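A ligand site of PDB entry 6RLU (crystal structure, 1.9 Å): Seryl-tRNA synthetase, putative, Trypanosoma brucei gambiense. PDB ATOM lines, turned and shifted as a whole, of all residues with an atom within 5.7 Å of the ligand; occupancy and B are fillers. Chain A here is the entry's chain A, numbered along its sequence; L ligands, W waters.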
ATOM      1  N   GLU A 248     -25.907 -26.343 -24.478  1.00  0.00           N
ATOM      2  CA  GLU A 248     -26.661 -26.186 -23.249  1.00  0.00           C
ATOM      3  C   GLU A 248     -28.044 -26.824 -23.179  1.00  0.00           C
ATOM      4  O   GLU A 248     -28.453 -27.222 -22.088  1.00  0.00           O
ATOM      5  CB  GLU A 248     -26.772 -24.656 -22.987  1.00  0.00           C
ATOM      6  CG  GLU A 248     -27.456 -24.200 -21.701  1.00  0.00           C
ATOM      7  CD  GLU A 248     -27.578 -22.685 -21.620  1.00  0.00           C
ATOM      8  OE1 GLU A 248     -28.135 -22.085 -22.567  1.00  0.00           O
ATOM      9  OE2 GLU A 248     -27.133 -22.105 -20.607  1.00  0.00           O
ATOM     10  N   ALA A 263     -32.994 -23.231 -19.704  1.00  0.00           N
ATOM     11  CA  ALA A 263     -31.713 -23.139 -18.983  1.00  0.00           C
ATOM     12  C   ALA A 263     -31.788 -22.089 -17.861  1.00  0.00           C
ATOM     13  O   ALA A 263     -30.877 -21.996 -17.050  1.00  0.00           O
ATOM     14  CB  ALA A 263     -30.614 -22.734 -19.974  1.00  0.00           C
ATOM     15  N   THR A 264     -32.854 -21.278 -17.861  1.00  0.00           N
ATOM     16  CA  THR A 264     -33.076 -20.179 -16.922  1.00  0.00           C
ATOM     17  C   THR A 264     -34.499 -19.678 -17.157  1.00  0.00           C
ATOM     18  O   THR A 264     -34.967 -19.725 -18.294  1.00  0.00           O
ATOM     19  CB  THR A 264     -32.061 -19.005 -17.196  1.00  0.00           C
ATOM     20  OG1 THR A 264     -32.534 -17.824 -16.530  1.00  0.00           O
ATOM     21  CG2 THR A 264     -31.818 -18.716 -18.697  1.00  0.00           C
ATOM     22  N   GLU A 266     -35.238 -16.731 -17.463  1.00  0.00           N
ATOM     23  CA  GLU A 266     -35.082 -15.585 -18.374  1.00  0.00           C
ATOM     24  C   GLU A 266     -35.666 -15.963 -19.771  1.00  0.00           C
ATOM     25  O   GLU A 266     -36.305 -15.127 -20.408  1.00  0.00           O
ATOM     26  CB  GLU A 266     -33.584 -15.235 -18.545  1.00  0.00           C
ATOM     27  CG  GLU A 266     -33.272 -14.262 -19.680  1.00  0.00           C
ATOM     28  CD  GLU A 266     -31.848 -14.331 -20.225  1.00  0.00           C
ATOM     29  OE1 GLU A 266     -30.960 -14.891 -19.556  1.00  0.00           O
ATOM     30  OE2 GLU A 266     -31.642 -13.830 -21.356  1.00  0.00           O
ATOM     31  N   ARG A 295     -29.227 -27.620 -17.843  1.00  0.00           N
ATOM     32  CA  ARG A 295     -28.088 -27.283 -18.726  1.00  0.00           C
ATOM     33  C   ARG A 295     -27.228 -28.483 -18.991  1.00  0.00           C
ATOM     34  O   ARG A 295     -26.776 -29.115 -18.048  1.00  0.00           O
ATOM     35  CB  ARG A 295     -27.229 -26.160 -18.116  1.00  0.00           C
ATOM     36  CG  ARG A 295     -28.024 -24.885 -17.844  1.00  0.00           C
ATOM     37  CD  ARG A 295     -27.146 -23.705 -17.501  1.00  0.00           C
ATOM     38  NE  ARG A 295     -28.006 -22.570 -17.169  1.00  0.00           N
ATOM     39  CZ  ARG A 295     -27.595 -21.313 -17.055  1.00  0.00           C
ATOM     40  NH1 ARG A 295     -26.301 -21.016 -17.225  1.00  0.00           N
ATOM     41  NH2 ARG A 295     -28.450 -20.350 -16.741  1.00  0.00           N
ATOM     42  N   GLU A 297     -24.232 -28.447 -20.048  1.00  0.00           N
ATOM     43  CA  GLU A 297     -22.859 -28.086 -19.671  1.00  0.00           C
ATOM     44  C   GLU A 297     -21.834 -28.774 -20.588  1.00  0.00           C
ATOM     45  O   GLU A 297     -20.854 -29.307 -20.096  1.00  0.00           O
ATOM     46  CB  GLU A 297     -22.592 -28.372 -18.166  1.00  0.00           C
ATOM     47  CG  GLU A 297     -23.417 -27.523 -17.205  1.00  0.00           C
ATOM     48  CD  GLU A 297     -23.090 -26.032 -17.233  1.00  0.00           C
ATOM     49  OE1 GLU A 297     -21.935 -25.676 -17.553  1.00  0.00           O
ATOM     50  OE2 GLU A 297     -23.994 -25.222 -16.927  1.00  0.00           O
ATOM     51  N   PHE A 309     -21.690 -27.743  -7.422  1.00  0.00           N
ATOM     52  CA  PHE A 309     -21.293 -26.414  -7.866  1.00  0.00           C
ATOM     53  C   PHE A 309     -21.737 -26.126  -9.327  1.00  0.00           C
ATOM     54  O   PHE A 309     -22.168 -25.017  -9.635  1.00  0.00           O
ATOM     55  CB  PHE A 309     -19.768 -26.257  -7.726  1.00  0.00           C
ATOM     56  CG  PHE A 309     -19.290 -24.882  -8.135  1.00  0.00           C
ATOM     57  CD1 PHE A 309     -19.285 -23.837  -7.222  1.00  0.00           C
ATOM     58  CD2 PHE A 309     -18.874 -24.626  -9.443  1.00  0.00           C
ATOM     59  CE1 PHE A 309     -18.861 -22.557  -7.598  1.00  0.00           C
ATOM     60  CE2 PHE A 309     -18.469 -23.350  -9.820  1.00  0.00           C
ATOM     61  CZ  PHE A 309     -18.462 -22.315  -8.897  1.00  0.00           C
ATOM     62  N   ARG A 310     -21.599 -27.122 -10.223  1.00  0.00           N
ATOM     63  CA  ARG A 310     -21.963 -26.982 -11.639  1.00  0.00           C
ATOM     64  C   ARG A 310     -22.662 -28.263 -12.092  1.00  0.00           C
ATOM     65  O   ARG A 310     -22.052 -29.186 -12.642  1.00  0.00           O
ATOM     66  CB  ARG A 310     -20.722 -26.646 -12.489  1.00  0.00           C
ATOM     67  CG  ARG A 310     -21.040 -26.270 -13.952  1.00  0.00           C
ATOM     68  CD  ARG A 310     -19.734 -26.118 -14.739  1.00  0.00           C
ATOM     69  NE  ARG A 310     -19.714 -24.884 -15.519  1.00  0.00           N
ATOM     70  N   VAL A 311     -23.956 -28.329 -11.821  1.00  0.00           N
ATOM     71  CA  VAL A 311     -24.752 -29.512 -12.162  1.00  0.00           C
ATOM     72  C   VAL A 311     -25.710 -29.212 -13.316  1.00  0.00           C
ATOM     73  O   VAL A 311     -25.851 -28.058 -13.714  1.00  0.00           O
ATOM     74  CB  VAL A 311     -25.480 -30.076 -10.908  1.00  0.00           C
ATOM     75  CG1 VAL A 311     -24.470 -30.735  -9.971  1.00  0.00           C
ATOM     76  CG2 VAL A 311     -26.265 -28.983 -10.175  1.00  0.00           C
ATOM     77  N   HIS A 312     -26.341 -30.259 -13.866  1.00  0.00           N
ATOM     78  CA  HIS A 312     -27.258 -30.064 -14.994  1.00  0.00           C
ATOM     79  C   HIS A 312     -28.591 -29.481 -14.551  1.00  0.00           C
ATOM     80  O   HIS A 312     -29.258 -28.869 -15.361  1.00  0.00           O
ATOM     81  CB  HIS A 312     -27.557 -31.403 -15.709  1.00  0.00           C
ATOM     82  CG  HIS A 312     -26.354 -32.078 -16.290  1.00  0.00           C
ATOM     83  ND1 HIS A 312     -25.636 -31.506 -17.323  1.00  0.00           N
ATOM     84  CD2 HIS A 312     -25.848 -33.293 -16.025  1.00  0.00           C
ATOM     85  CE1 HIS A 312     -24.678 -32.377 -17.620  1.00  0.00           C
ATOM     86  NE2 HIS A 312     -24.767 -33.472 -16.865  1.00  0.00           N
ATOM     87  N   PHE A 314     -30.804 -27.437 -11.497  1.00  0.00           N
ATOM     88  CA  PHE A 314     -30.703 -26.557 -10.329  1.00  0.00           C
ATOM     89  C   PHE A 314     -31.798 -25.518 -10.299  1.00  0.00           C
ATOM     90  O   PHE A 314     -32.222 -25.049 -11.349  1.00  0.00           O
ATOM     91  CB  PHE A 314     -29.298 -25.847 -10.285  1.00  0.00           C
ATOM     92  CG  PHE A 314     -28.968 -24.950 -11.474  1.00  0.00           C
ATOM     93  CD1 PHE A 314     -29.105 -23.561 -11.379  1.00  0.00           C
ATOM     94  CD2 PHE A 314     -28.494 -25.494 -12.669  1.00  0.00           C
ATOM     95  CE1 PHE A 314     -28.795 -22.734 -12.471  1.00  0.00           C
ATOM     96  CE2 PHE A 314     -28.203 -24.671 -13.762  1.00  0.00           C
ATOM     97  CZ  PHE A 314     -28.367 -23.298 -13.659  1.00  0.00           C
ATOM     98  N   LYS A 316     -33.181 -21.717  -9.589  1.00  0.00           N
ATOM     99  CA  LYS A 316     -32.671 -20.359  -9.678  1.00  0.00           C
ATOM    100  C   LYS A 316     -33.842 -19.361  -9.561  1.00  0.00           C
ATOM    101  O   LYS A 316     -34.874 -19.537 -10.209  1.00  0.00           O
ATOM    102  CB  LYS A 316     -31.851 -20.133 -10.966  1.00  0.00           C
ATOM    103  CG  LYS A 316     -31.298 -18.684 -11.069  1.00  0.00           C
ATOM    104  CD  LYS A 316     -30.311 -18.448 -12.252  1.00  0.00           C
ATOM    105  CE  LYS A 316     -30.872 -18.791 -13.627  1.00  0.00           C
ATOM    106  NZ  LYS A 316     -32.186 -18.123 -13.881  1.00  0.00           N
ATOM    107  N   GLU A 318     -34.704 -15.489 -10.315  1.00  0.00           N
ATOM    108  CA  GLU A 318     -34.247 -14.542 -11.338  1.00  0.00           C
ATOM    109  C   GLU A 318     -34.929 -13.185 -11.260  1.00  0.00           C
ATOM    110  O   GLU A 318     -36.143 -13.128 -11.080  1.00  0.00           O
ATOM    111  CB  GLU A 318     -34.637 -15.178 -12.692  1.00  0.00           C
ATOM    112  CG  GLU A 318     -34.239 -14.447 -13.947  1.00  0.00           C
ATOM    113  CD  GLU A 318     -32.770 -14.515 -14.310  1.00  0.00           C
ATOM    114  OE1 GLU A 318     -32.419 -14.036 -15.408  1.00  0.00           O
ATOM    115  OE2 GLU A 318     -31.966 -15.047 -13.502  1.00  0.00           O
ATOM    116  N   GLU A 384     -18.124 -17.042  -9.579  1.00  0.00           N
ATOM    117  CA  GLU A 384     -19.332 -16.443 -10.084  1.00  0.00           C
ATOM    118  C   GLU A 384     -20.599 -17.062  -9.429  1.00  0.00           C
ATOM    119  O   GLU A 384     -20.774 -18.283  -9.474  1.00  0.00           O
ATOM    120  CB  GLU A 384     -19.358 -16.679 -11.609  1.00  0.00           C
ATOM    121  CG  GLU A 384     -20.571 -16.072 -12.314  1.00  0.00           C
ATOM    122  CD  GLU A 384     -20.822 -16.626 -13.700  1.00  0.00           C
ATOM    123  OE1 GLU A 384     -19.860 -17.114 -14.338  1.00  0.00           O
ATOM    124  OE2 GLU A 384     -21.991 -16.574 -14.151  1.00  0.00           O
ATOM    125  N   LEU A 385     -21.461 -16.215  -8.830  1.00  0.00           N
ATOM    126  CA  LEU A 385     -22.771 -16.642  -8.317  1.00  0.00           C
ATOM    127  C   LEU A 385     -23.879 -15.979  -9.116  1.00  0.00           C
ATOM    128  O   LEU A 385     -25.001 -16.477  -9.142  1.00  0.00           O
ATOM    129  CB  LEU A 385     -22.986 -16.220  -6.829  1.00  0.00           C
ATOM    130  CG  LEU A 385     -22.277 -16.990  -5.726  1.00  0.00           C
ATOM    131  CD1 LEU A 385     -22.929 -16.704  -4.368  1.00  0.00           C
ATOM    132  CD2 LEU A 385     -22.306 -18.489  -5.961  1.00  0.00           C
ATOM    133  N   VAL A 386     -23.584 -14.779  -9.670  1.00  0.00           N
ATOM    134  CA  VAL A 386     -24.593 -13.929 -10.317  1.00  0.00           C
ATOM    135  C   VAL A 386     -24.060 -13.262 -11.571  1.00  0.00           C
ATOM    136  O   VAL A 386     -22.933 -12.783 -11.566  1.00  0.00           O
ATOM    137  CB  VAL A 386     -24.975 -12.764  -9.298  1.00  0.00           C
ATOM    138  CG1 VAL A 386     -25.757 -11.620  -9.965  1.00  0.00           C
ATOM    139  CG2 VAL A 386     -25.705 -13.267  -8.042  1.00  0.00           C
ATOM    140  N   SER A 387     -24.943 -13.105 -12.580  1.00  0.00           N
ATOM    141  CA  SER A 387     -24.713 -12.271 -13.744  1.00  0.00           C
ATOM    142  C   SER A 387     -25.935 -11.375 -13.864  1.00  0.00           C
ATOM    143  O   SER A 387     -27.082 -11.871 -13.800  1.00  0.00           O
ATOM    144  CB  SER A 387     -24.556 -13.092 -15.022  1.00  0.00           C
ATOM    145  OG  SER A 387     -23.307 -13.741 -15.059  1.00  0.00           O
ATOM    146  N   CYS A 388     -25.708 -10.061 -14.063  1.00  0.00           N
ATOM    147  CA  CYS A 388     -26.771  -9.037 -14.243  1.00  0.00           C
ATOM    148  C   CYS A 388     -26.452  -8.312 -15.540  1.00  0.00           C
ATOM    149  O   CYS A 388     -25.392  -7.688 -15.630  1.00  0.00           O
ATOM    150  CB  CYS A 388     -26.800  -8.021 -13.082  1.00  0.00           C
ATOM    151  SG  CYS A 388     -27.632  -8.575 -11.590  1.00  0.00           S
ATOM    152  N   ASN A 423     -31.937  -8.794 -17.269  1.00  0.00           N
ATOM    153  CA  ASN A 423     -32.059 -10.029 -16.502  1.00  0.00           C
ATOM    154  C   ASN A 423     -30.875 -10.100 -15.551  1.00  0.00           C
ATOM    155  O   ASN A 423     -29.776  -9.622 -15.868  1.00  0.00           O
ATOM    156  CB  ASN A 423     -32.165 -11.279 -17.408  1.00  0.00           C
ATOM    157  CG  ASN A 423     -30.899 -11.586 -18.150  1.00  0.00           C
ATOM    158  OD1 ASN A 423     -29.990 -12.228 -17.615  1.00  0.00           O
ATOM    159  ND2 ASN A 423     -30.781 -11.090 -19.364  1.00  0.00           N
ATOM    160  N   GLY A 424     -31.123 -10.652 -14.384  1.00  0.00           N
ATOM    161  CA  GLY A 424     -30.075 -10.764 -13.378  1.00  0.00           C
ATOM    162  C   GLY A 424     -30.360 -11.849 -12.368  1.00  0.00           C
ATOM    163  O   GLY A 424     -31.459 -11.917 -11.831  1.00  0.00           O
ATOM    164  N   THR A 425     -29.352 -12.674 -12.090  1.00  0.00           N
ATOM    165  CA  THR A 425     -29.521 -13.723 -11.095  1.00  0.00           C
ATOM    166  C   THR A 425     -29.798 -13.073  -9.749  1.00  0.00           C
ATOM    167  O   THR A 425     -29.124 -12.100  -9.381  1.00  0.00           O
ATOM    168  CB  THR A 425     -28.200 -14.509 -10.937  1.00  0.00           C
ATOM    169  OG1 THR A 425     -27.666 -14.781 -12.217  1.00  0.00           O
ATOM    170  CG2 THR A 425     -28.371 -15.805 -10.144  1.00  0.00           C
ATOM    171  N   LEU A 426     -30.729 -13.658  -8.972  1.00  0.00           N
ATOM    172  CA  LEU A 426     -30.861 -13.225  -7.572  1.00  0.00           C
ATOM    173  C   LEU A 426     -30.202 -14.340  -6.758  1.00  0.00           C
ATOM    174  O   LEU A 426     -29.298 -14.064  -5.968  1.00  0.00           O
ATOM    175  CB  LEU A 426     -32.330 -12.966  -7.160  1.00  0.00           C
ATOM    176  CG  LEU A 426     -32.607 -12.379  -5.766  1.00  0.00           C
ATOM    177  CD1 LEU A 426     -32.671 -13.451  -4.699  1.00  0.00           C
ATOM    178  CD2 LEU A 426     -31.651 -11.184  -5.400  1.00  0.00           C
ATOM    179  N   ALA A 428     -28.786 -18.504  -7.444  1.00  0.00           N
ATOM    180  CA  ALA A 428     -28.613 -19.820  -8.086  1.00  0.00           C
ATOM    181  C   ALA A 428     -28.436 -20.706  -6.842  1.00  0.00           C
ATOM    182  O   ALA A 428     -27.447 -20.584  -6.108  1.00  0.00           O
ATOM    183  CB  ALA A 428     -27.379 -19.842  -8.964  1.00  0.00           C
ATOM    184  N   THR A 430     -28.132 -24.153  -5.832  1.00  0.00           N
ATOM    185  CA  THR A 430     -27.077 -25.125  -5.460  1.00  0.00           C
ATOM    186  C   THR A 430     -25.729 -24.465  -5.260  1.00  0.00           C
ATOM    187  O   THR A 430     -24.998 -24.814  -4.315  1.00  0.00           O
ATOM    188  CB  THR A 430     -27.011 -26.358  -6.410  1.00  0.00           C
ATOM    189  OG1 THR A 430     -26.584 -25.957  -7.711  1.00  0.00           O
ATOM    190  CG2 THR A 430     -28.334 -27.110  -6.495  1.00  0.00           C
ATOM    191  N   ARG A 431     -25.404 -23.502  -6.114  1.00  0.00           N
ATOM    192  CA  ARG A 431     -24.121 -22.811  -5.984  1.00  0.00           C
ATOM    193  C   ARG A 431     -24.062 -21.944  -4.728  1.00  0.00           C
ATOM    194  O   ARG A 431     -23.022 -21.909  -4.066  1.00  0.00           O
ATOM    195  CB  ARG A 431     -23.774 -22.029  -7.258  1.00  0.00           C
ATOM    196  CG  ARG A 431     -22.308 -21.742  -7.333  1.00  0.00           C
ATOM    197  CD  ARG A 431     -21.932 -21.095  -8.643  1.00  0.00           C
ATOM    198  NE  ARG A 431     -21.927 -22.059  -9.732  1.00  0.00           N
ATOM    199  CZ  ARG A 431     -21.455 -21.795 -10.948  1.00  0.00           C
ATOM    200  NH1 ARG A 431     -20.956 -20.596 -11.226  1.00  0.00           N
ATOM    201  NH2 ARG A 431     -21.484 -22.722 -11.876  1.00  0.00           N
HETATM  202  O1  LIG L   1     -25.967 -18.200 -17.387  1.00  0.00           O
HETATM  203  O2  LIG L   1     -24.744 -16.684 -15.846  1.00  0.00           O
HETATM  204  N1  LIG L   1     -30.636 -15.420 -16.899  1.00  0.00           N
HETATM  205  C1  LIG L   1     -29.236 -15.082 -16.573  1.00  0.00           C
HETATM  206  C2  LIG L   1     -28.414 -16.342 -16.582  1.00  0.00           C
HETATM  207  O3  LIG L   1     -28.870 -17.485 -16.671  1.00  0.00           O
HETATM  208  C3  LIG L   1     -29.106 -14.377 -15.222  1.00  0.00           C
HETATM  209  O4  LIG L   1     -29.440 -15.240 -14.133  1.00  0.00           O
HETATM  210  C4  LIG L   1     -25.386 -20.290 -11.935  1.00  0.00           C
HETATM  211  C5  LIG L   1     -25.273 -22.748 -11.763  1.00  0.00           C
HETATM  212  C6  LIG L   1     -24.134 -19.377 -11.905  1.00  0.00           C
HETATM  213  C7  LIG L   1     -24.546 -18.206 -12.820  1.00  0.00           C
HETATM  214  C8  LIG L   1     -24.843 -24.090 -13.640  1.00  0.00           C
HETATM  215  C9  LIG L   1     -26.064 -18.200 -12.682  1.00  0.00           C
HETATM  216  C10 LIG L   1     -24.691 -22.938 -14.480  1.00  0.00           C
HETATM  217  C11 LIG L   1     -26.811 -17.540 -13.812  1.00  0.00           C
HETATM  218  C12 LIG L   1     -24.882 -21.725 -13.905  1.00  0.00           C
HETATM  219  N2  LIG L   1     -25.171 -21.608 -12.565  1.00  0.00           N
HETATM  220  N3  LIG L   1     -25.113 -23.968 -12.329  1.00  0.00           N
HETATM  221  N4  LIG L   1     -27.019 -16.138 -16.483  1.00  0.00           N
HETATM  222  N5  LIG L   1     -24.776 -25.311 -14.159  1.00  0.00           N
HETATM  223  O5  LIG L   1     -25.440 -22.610 -10.549  1.00  0.00           O
HETATM  224  O6  LIG L   1     -23.892 -18.965 -10.566  1.00  0.00           O
HETATM  225  O7  LIG L   1     -24.013 -16.946 -12.433  1.00  0.00           O
HETATM  226  O8  LIG L   1     -26.420 -19.605 -12.631  1.00  0.00           O
HETATM  227  O9  LIG L   1     -26.423 -18.203 -15.046  1.00  0.00           O
HETATM  228  S1  LIG L   1     -25.949 -17.304 -16.280  1.00  0.00           S
HETATM  229  O   HOH W   1     -27.010 -23.405  -8.488  1.00  0.00           O
HETATM  230  O   HOH W   2     -23.303 -14.782 -18.115  1.00  0.00           O
HETATM  231  O   HOH W   3     -22.225 -17.356 -17.722  1.00  0.00           O
HETATM  232  O   HOH W   4     -25.031 -25.969 -10.342  1.00  0.00           O
HETATM  233  O   HOH W   5     -26.009 -13.918 -18.018  1.00  0.00           O
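Water W1 lies within hydrogen-bond range of the side-chain hydroxyl (OG1) of Thr 430 (2.7 Å), an oxygen (O5) of the ligand (2.7 Å) and the backbone NH (N) of Arg 431 (2.9 Å).
Water W4 lies within hydrogen-bond range of N3 of the ligand, N of Val 311, OG1 of Thr 430 and O of Phe 309.
Water W2 lies within hydrogen-bond range of OG of Ser 387 (3.2 Å) and O2 of the ligand (3.3 Å).
Residues that only touch the ligand: Phe 314 (3.4 Å), Val 386 (3.5 Å), Ala 428 (3.6 Å), Lys 316 (3.8 Å), Arg 310 (3.9 Å) and Gly 424 (3.9 Å).
Hydrophobic or aromatic side chains within 4 Å of the ligand: Phe 314 and Ala 428.
Of the 25 residues printed, 18 come within 4 Å of the ligand.
The nearest printed residue that does not touch the ligand is Phe 309 (4.1 Å).
The backbone carbonyl oxygen (O) of Glu 384 is in hydrogen-bond range of an oxygen (O6) of the ligand (3.4 Å).
The side-chain hydroxyl (OG1) of Thr 264 sits at hydrogen-bond distance from a nitrogen (N1) of the ligand (3.1 Å).
OE2 of Glu 384 is in hydrogen-bond range of O7 of the ligand, at 2.7 Å.
O of Leu 385 sits at hydrogen-bond distance from O6 of the ligand, 3.1 Å away.
The guanidinium group (NH1) of Arg 431 lies within hydrogen-bond range of an oxygen (O6) of the ligand (3.4 Å).
A nitrogen (N1) of the ligand sits close to the side-chain amide oxygen of Asn 423.
A nitrogen (N1) of the ligand is in salt-bridge range of the side-chain carboxylate (OE1) of Glu 266, 2.7 Å away.
O4 of the ligand sits at hydrogen-bond distance from OG1 of Thr 425 (2.7 Å).
An oxygen (O1) of the ligand sits at hydrogen-bond distance from the guanidinium group of Arg 295 (2.8 Å).
A nitrogen (N5) of the ligand lies within hydrogen-bond range of the backbone carbonyl oxygen of Val 311, at 3.0 Å.
The side-chain hydroxyl (OG) of Ser 387 is in hydrogen-bond range of an oxygen (O2) of the ligand, 3.4 Å away.
The side-chain carboxylate (OE1) of Glu 318 is in salt-bridge range of a nitrogen (N1) of the ligand (2.7 Å).
A nitrogen (N5) of the ligand lies within hydrogen-bond range of the side-chain carboxylate (OE2) of Glu 297 (2.9 Å).
The backbone NH (N) of Thr 425 lies within hydrogen-bond range of an oxygen (O4) of the ligand.
OG1 of Thr 264 sits at hydrogen-bond distance from NZ of Lys 316.
OE2 of Glu 384 sits at hydrogen-bond distance from OG of Ser 387 (3.3 Å).
The side-chain hydroxyl (OG1) of Thr 264 sits close to the backbone NH (N) of Glu 266 (3.1 Å).
OE1 of Glu 266 lies close to OD1 of Asn 423 (3.4 Å).
ND1 of His 312 sits at hydrogen-bond distance from O of Arg 295, at 2.7 Å.
OE2 of Glu 318 is in salt-bridge range of NZ of Lys 316, 3.1 Å away.
The backbone carbonyl oxygen of Glu 384 sits at hydrogen-bond distance from the guanidinium group of Arg 431, 2.9 Å away.
N of Thr 425 is in hydrogen-bond range of O of Ser 387.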
